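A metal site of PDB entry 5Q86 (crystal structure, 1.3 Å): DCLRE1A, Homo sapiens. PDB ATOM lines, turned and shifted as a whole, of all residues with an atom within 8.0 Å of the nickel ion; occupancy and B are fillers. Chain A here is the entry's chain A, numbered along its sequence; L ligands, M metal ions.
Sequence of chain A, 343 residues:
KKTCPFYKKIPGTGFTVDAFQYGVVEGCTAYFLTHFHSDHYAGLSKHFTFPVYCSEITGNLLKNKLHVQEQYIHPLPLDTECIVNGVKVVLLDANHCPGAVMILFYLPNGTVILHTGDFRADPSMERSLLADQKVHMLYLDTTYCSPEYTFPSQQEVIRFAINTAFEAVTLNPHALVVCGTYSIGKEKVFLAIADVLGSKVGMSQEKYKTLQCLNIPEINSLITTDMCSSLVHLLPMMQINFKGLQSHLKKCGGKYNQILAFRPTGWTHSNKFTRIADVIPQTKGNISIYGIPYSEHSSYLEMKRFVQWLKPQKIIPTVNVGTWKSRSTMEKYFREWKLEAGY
NE2 of His 37 is in hydrogen-bond range of O of Ile 184, 2.9 Å away. A ring nitrogen (ND1) of His 35 is in hydrogen-bond range of the side-chain hydroxyl (OG1) of Thr 34. OD2 of Asp 118 sits close to NE2 of His 40, 3.3 Å away. ND1 of His 96 lies within hydrogen-bond range of O of Glu 296 (2.8 Å).
The nearest printed residue that does not touch the nickel ion is His 40 (4.3 Å).
The nickel ion is bound by an oxygen (O3) of the ligand (2.1 Å), an oxygen (O2) of the ligand (2.2 Å), a ring nitrogen (ND1) of His 37 (2.2 Å), a ring nitrogen (NE2) of His 35 (2.2 Å), the side-chain carboxylate of Asp 118 (2.2 Å) and a ring nitrogen (NE2) of His 96 (2.3 Å). The nickel ion has six donor atoms within binding distance.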
ATOM      1  N   ASP A  18     -11.041  -2.427  35.794  1.00  0.00           N
ATOM      2  CA  ASP A  18      -9.982  -3.046  34.953  1.00  0.00           C
ATOM      3  C   ASP A  18      -8.988  -3.914  35.825  1.00  0.00           C
ATOM      4  O   ASP A  18      -7.744  -3.845  35.632  1.00  0.00           O
ATOM      5  CB  ASP A  18      -9.314  -2.021  34.059  1.00  0.00           C
ATOM      6  CG  ASP A  18     -10.277  -1.303  33.105  1.00  0.00           C
ATOM      7  OD1 ASP A  18     -11.437  -1.761  32.959  1.00  0.00           O
ATOM      8  OD2 ASP A  18      -9.812  -0.276  32.509  1.00  0.00           O
ATOM      9  N   THR A  34     -13.691  -1.029  31.432  1.00  0.00           N
ATOM     10  CA  THR A  34     -13.862   0.172  30.630  1.00  0.00           C
ATOM     11  C   THR A  34     -13.932  -0.110  29.112  1.00  0.00           C
ATOM     12  O   THR A  34     -14.671   0.604  28.406  1.00  0.00           O
ATOM     13  CB  THR A  34     -12.784   1.220  30.933  1.00  0.00           C
ATOM     14  OG1 THR A  34     -11.477   0.698  30.560  1.00  0.00           O
ATOM     15  CG2 THR A  34     -12.812   1.695  32.374  1.00  0.00           C
ATOM     16  N   HIS A  35     -13.147  -1.128  28.657  1.00  0.00           N
ATOM     17  CA  HIS A  35     -13.044  -1.414  27.239  1.00  0.00           C
ATOM     18  C   HIS A  35     -12.405  -2.765  27.003  1.00  0.00           C
ATOM     19  O   HIS A  35     -11.638  -3.226  27.887  1.00  0.00           O
ATOM     20  CB  HIS A  35     -12.376  -0.236  26.457  1.00  0.00           C
ATOM     21  CG  HIS A  35     -10.916  -0.043  26.697  1.00  0.00           C
ATOM     22  ND1 HIS A  35     -10.384   0.418  27.891  1.00  0.00           N
ATOM     23  CD2 HIS A  35      -9.871  -0.221  25.870  1.00  0.00           C
ATOM     24  CE1 HIS A  35      -9.065   0.574  27.717  1.00  0.00           C
ATOM     25  NE2 HIS A  35      -8.756   0.227  26.510  1.00  0.00           N
ATOM     26  N   PHE A  36     -12.613  -3.266  25.785  1.00  0.00           N
ATOM     27  CA  PHE A  36     -12.039  -4.628  25.412  1.00  0.00           C
ATOM     28  C   PHE A  36     -10.667  -4.531  24.790  1.00  0.00           C
ATOM     29  O   PHE A  36     -10.511  -4.815  23.558  1.00  0.00           O
ATOM     30  CB  PHE A  36     -13.062  -5.319  24.440  1.00  0.00           C
ATOM     31  CG  PHE A  36     -12.827  -6.835  24.257  1.00  0.00           C
ATOM     32  CD1 PHE A  36     -13.168  -7.695  25.302  1.00  0.00           C
ATOM     33  CD2 PHE A  36     -12.247  -7.338  23.095  1.00  0.00           C
ATOM     34  CE1 PHE A  36     -13.005  -9.082  25.123  1.00  0.00           C
ATOM     35  CE2 PHE A  36     -12.031  -8.716  22.937  1.00  0.00           C
ATOM     36  CZ  PHE A  36     -12.402  -9.539  23.927  1.00  0.00           C
ATOM     37  N   HIS A  37      -9.648  -4.123  25.566  1.00  0.00           N
ATOM     38  CA  HIS A  37      -8.220  -4.217  25.211  1.00  0.00           C
ATOM     39  C   HIS A  37      -7.567  -5.140  26.238  1.00  0.00           C
ATOM     40  O   HIS A  37      -7.867  -5.078  27.458  1.00  0.00           O
ATOM     41  CB  HIS A  37      -7.534  -2.828  25.185  1.00  0.00           C
ATOM     42  CG  HIS A  37      -7.724  -2.043  23.905  1.00  0.00           C
ATOM     43  ND1 HIS A  37      -7.437  -0.697  23.789  1.00  0.00           N
ATOM     44  CD2 HIS A  37      -8.142  -2.438  22.688  1.00  0.00           C
ATOM     45  CE1 HIS A  37      -7.644  -0.286  22.542  1.00  0.00           C
ATOM     46  NE2 HIS A  37      -8.069  -1.340  21.870  1.00  0.00           N
ATOM     47  N   SER A  38      -6.634  -5.961  25.768  1.00  0.00           N
ATOM     48  CA  SER A  38      -6.129  -7.093  26.570  1.00  0.00           C
ATOM     49  C   SER A  38      -5.437  -6.664  27.838  1.00  0.00           C
ATOM     50  O   SER A  38      -5.571  -7.410  28.820  1.00  0.00           O
ATOM     51  CB  SER A  38      -5.313  -8.070  25.693  1.00  0.00           C
ATOM     52  OG  SER A  38      -4.153  -7.440  25.207  1.00  0.00           O
ATOM     53  N   ASP A  39      -4.705  -5.547  27.898  1.00  0.00           N
ATOM     54  CA  ASP A  39      -4.065  -5.118  29.194  1.00  0.00           C
ATOM     55  C   ASP A  39      -5.140  -4.833  30.258  1.00  0.00           C
ATOM     56  O   ASP A  39      -4.855  -4.883  31.457  1.00  0.00           O
ATOM     57  CB  ASP A  39      -3.205  -3.902  29.011  1.00  0.00           C
ATOM     58  CG  ASP A  39      -1.770  -4.189  28.406  1.00  0.00           C
ATOM     59  OD1 ASP A  39      -1.426  -5.368  28.186  1.00  0.00           O
ATOM     60  OD2 ASP A  39      -1.090  -3.186  28.144  1.00  0.00           O
ATOM     61  N   HIS A  40      -6.373  -4.468  29.849  1.00  0.00           N
ATOM     62  CA  HIS A  40      -7.469  -4.136  30.747  1.00  0.00           C
ATOM     63  C   HIS A  40      -8.357  -5.293  31.096  1.00  0.00           C
ATOM     64  O   HIS A  40      -8.752  -5.411  32.296  1.00  0.00           O
ATOM     65  CB  HIS A  40      -8.259  -2.943  30.092  1.00  0.00           C
ATOM     66  CG  HIS A  40      -7.414  -1.728  29.946  1.00  0.00           C
ATOM     67  ND1 HIS A  40      -7.504  -0.639  30.791  1.00  0.00           N
ATOM     68  CD2 HIS A  40      -6.450  -1.403  29.051  1.00  0.00           C
ATOM     69  CE1 HIS A  40      -6.633   0.288  30.429  1.00  0.00           C
ATOM     70  NE2 HIS A  40      -5.963  -0.165  29.381  1.00  0.00           N
ATOM     71  N   HIS A  96     -12.357   6.395  22.435  1.00  0.00           N
ATOM     72  CA  HIS A  96     -11.175   5.448  22.351  1.00  0.00           C
ATOM     73  C   HIS A  96     -11.535   4.440  21.278  1.00  0.00           C
ATOM     74  O   HIS A  96     -11.653   4.922  20.089  1.00  0.00           O
ATOM     75  CB  HIS A  96     -10.826   4.924  23.758  1.00  0.00           C
ATOM     76  CG  HIS A  96      -9.597   4.028  23.869  1.00  0.00           C
ATOM     77  ND1 HIS A  96      -8.369   4.395  23.389  1.00  0.00           N
ATOM     78  CD2 HIS A  96      -9.462   2.777  24.376  1.00  0.00           C
ATOM     79  CE1 HIS A  96      -7.498   3.413  23.637  1.00  0.00           C
ATOM     80  NE2 HIS A  96      -8.127   2.424  24.218  1.00  0.00           N
ATOM     81  N   CYS A  97     -11.683   3.177  21.556  1.00  0.00           N
ATOM     82  CA  CYS A  97     -12.119   2.149  20.611  1.00  0.00           C
ATOM     83  C   CYS A  97     -13.615   1.875  20.757  1.00  0.00           C
ATOM     84  O   CYS A  97     -14.235   2.397  21.711  1.00  0.00           O
ATOM     85  CB  CYS A  97     -11.273   0.875  20.873  1.00  0.00           C
ATOM     86  SG  CYS A  97     -11.566   0.112  22.531  1.00  0.00           S
ATOM     87  N   ALA A 100     -15.721   1.648  24.351  1.00  0.00           N
ATOM     88  CA  ALA A 100     -14.918   2.220  25.448  1.00  0.00           C
ATOM     89  C   ALA A 100     -15.658   3.292  26.180  1.00  0.00           C
ATOM     90  O   ALA A 100     -16.264   4.183  25.529  1.00  0.00           O
ATOM     91  CB  ALA A 100     -13.586   2.750  24.965  1.00  0.00           C
ATOM     92  N   GLY A 117     -10.924   5.642  32.070  1.00  0.00           N
ATOM     93  CA  GLY A 117     -10.451   4.511  31.320  1.00  0.00           C
ATOM     94  C   GLY A 117      -9.309   4.937  30.413  1.00  0.00           C
ATOM     95  O   GLY A 117      -8.546   5.817  30.773  1.00  0.00           O
ATOM     96  N   ASP A 118      -9.250   4.364  29.213  1.00  0.00           N
ATOM     97  CA  ASP A 118      -8.456   4.932  28.117  1.00  0.00           C
ATOM     98  C   ASP A 118      -9.343   5.918  27.315  1.00  0.00           C
ATOM     99  O   ASP A 118     -10.522   5.606  27.030  1.00  0.00           O
ATOM    100  CB  ASP A 118      -7.896   3.885  27.167  1.00  0.00           C
ATOM    101  CG  ASP A 118      -6.671   3.090  27.719  1.00  0.00           C
ATOM    102  OD1 ASP A 118      -6.078   3.472  28.726  1.00  0.00           O
ATOM    103  OD2 ASP A 118      -6.276   2.148  27.009  1.00  0.00           O
ATOM    104  N   PHE A 119      -8.824   7.111  26.997  1.00  0.00           N
ATOM    105  CA  PHE A 119      -9.664   8.120  26.264  1.00  0.00           C
ATOM    106  C   PHE A 119      -8.791   9.002  25.369  1.00  0.00           C
ATOM    107  O   PHE A 119      -7.613   9.177  25.581  1.00  0.00           O
ATOM    108  CB  PHE A 119     -10.581   8.971  27.250  1.00  0.00           C
ATOM    109  CG  PHE A 119      -9.977  10.210  27.945  1.00  0.00           C
ATOM    110  CD1 PHE A 119     -10.721  11.339  28.132  1.00  0.00           C
ATOM    111  CD2 PHE A 119      -8.679  10.208  28.489  1.00  0.00           C
ATOM    112  CE1 PHE A 119     -10.247  12.464  28.792  1.00  0.00           C
ATOM    113  CE2 PHE A 119      -8.165  11.341  29.163  1.00  0.00           C
ATOM    114  CZ  PHE A 119      -8.975  12.467  29.310  1.00  0.00           C
ATOM    115  N   ASP A 141      -6.136   8.756  32.239  1.00  0.00           N
ATOM    116  CA  ASP A 141      -5.265   8.107  31.197  1.00  0.00           C
ATOM    117  C   ASP A 141      -4.226   9.138  30.783  1.00  0.00           C
ATOM    118  O   ASP A 141      -4.458  10.111  30.051  1.00  0.00           O
ATOM    119  CB  ASP A 141      -6.096   7.703  29.997  1.00  0.00           C
ATOM    120  CG  ASP A 141      -5.297   7.310  28.767  1.00  0.00           C
ATOM    121  OD1 ASP A 141      -4.075   7.109  28.916  1.00  0.00           O
ATOM    122  OD2 ASP A 141      -5.883   7.251  27.648  1.00  0.00           O
ATOM    123  N   THR A 143      -1.294   8.376  29.181  1.00  0.00           N
ATOM    124  CA  THR A 143      -0.379   7.740  28.226  1.00  0.00           C
ATOM    125  C   THR A 143       0.582   8.717  27.587  1.00  0.00           C
ATOM    126  O   THR A 143       1.820   8.437  27.593  1.00  0.00           O
ATOM    127  CB  THR A 143      -1.234   7.005  27.103  1.00  0.00           C
ATOM    128  OG1 THR A 143      -2.000   5.955  27.635  1.00  0.00           O
ATOM    129  CG2 THR A 143      -0.284   6.398  26.046  1.00  0.00           C
ATOM    130  N   SER A 183      -5.939  -5.478  17.591  1.00  0.00           N
ATOM    131  CA  SER A 183      -6.903  -5.266  18.629  1.00  0.00           C
ATOM    132  C   SER A 183      -8.065  -4.514  17.960  1.00  0.00           C
ATOM    133  O   SER A 183      -7.942  -4.017  16.798  1.00  0.00           O
ATOM    134  CB  SER A 183      -6.334  -4.377  19.745  1.00  0.00           C
ATOM    135  OG  SER A 183      -6.010  -3.086  19.233  1.00  0.00           O
ATOM    136  N   ILE A 184      -9.168  -4.349  18.667  1.00  0.00           N
ATOM    137  CA  ILE A 184     -10.175  -3.426  18.194  1.00  0.00           C
ATOM    138  C   ILE A 184      -9.704  -1.968  18.322  1.00  0.00           C
ATOM    139  O   ILE A 184      -8.702  -1.647  19.065  1.00  0.00           O
ATOM    140  CB  ILE A 184     -11.559  -3.570  18.927  1.00  0.00           C
ATOM    141  CG1 ILE A 184     -11.514  -3.221  20.401  1.00  0.00           C
ATOM    142  CG2 ILE A 184     -12.051  -5.001  18.663  1.00  0.00           C
ATOM    143  CD1 ILE A 184     -12.845  -3.053  21.082  1.00  0.00           C
ATOM    144  N   GLU A 296      -5.745   6.910  19.318  1.00  0.00           N
ATOM    145  CA  GLU A 296      -6.963   6.842  20.157  1.00  0.00           C
ATOM    146  C   GLU A 296      -6.727   7.218  21.643  1.00  0.00           C
ATOM    147  O   GLU A 296      -7.549   6.914  22.520  1.00  0.00           O
ATOM    148  CB  GLU A 296      -7.715   5.530  19.986  1.00  0.00           C
ATOM    149  CG  GLU A 296      -8.359   5.356  18.529  1.00  0.00           C
ATOM    150  CD  GLU A 296      -9.247   4.130  18.301  1.00  0.00           C
ATOM    151  OE1 GLU A 296      -9.133   3.129  19.040  1.00  0.00           O
ATOM    152  OE2 GLU A 296     -10.028   4.189  17.278  1.00  0.00           O
ATOM    153  N   HIS A 297      -5.599   7.902  21.855  1.00  0.00           N
ATOM    154  CA  HIS A 297      -5.334   8.541  23.178  1.00  0.00           C
ATOM    155  C   HIS A 297      -5.114  10.064  23.047  1.00  0.00           C
ATOM    156  O   HIS A 297      -4.652  10.560  21.975  1.00  0.00           O
ATOM    157  CB  HIS A 297      -4.044   7.961  23.872  1.00  0.00           C
ATOM    158  CG  HIS A 297      -4.103   6.517  24.238  1.00  0.00           C
ATOM    159  ND1 HIS A 297      -4.611   6.073  25.439  1.00  0.00           N
ATOM    160  CD2 HIS A 297      -3.675   5.377  23.590  1.00  0.00           C
ATOM    161  CE1 HIS A 297      -4.555   4.746  25.499  1.00  0.00           C
ATOM    162  NE2 HIS A 297      -3.980   4.330  24.392  1.00  0.00           N
HETATM  163  C1  LIG L   1      -3.984  -0.416  24.433  1.00  0.00           C
HETATM  164  C2  LIG L   1      -4.134   1.051  24.034  1.00  0.00           C
HETATM  165  C3  LIG L   1      -4.459  -0.770  25.844  1.00  0.00           C
HETATM  166  O1  LIG L   1      -3.257   1.811  23.621  1.00  0.00           O
HETATM  167  O2  LIG L   1      -5.218   1.531  24.219  1.00  0.00           O
HETATM  168  O3  LIG L   1      -5.587  -0.451  26.232  1.00  0.00           O
HETATM  169  O4  LIG L   1      -3.752  -1.549  26.536  1.00  0.00           O
HETATM  170 NI    NI M   1      -6.945   0.820  25.337  1.00  0.00          NI
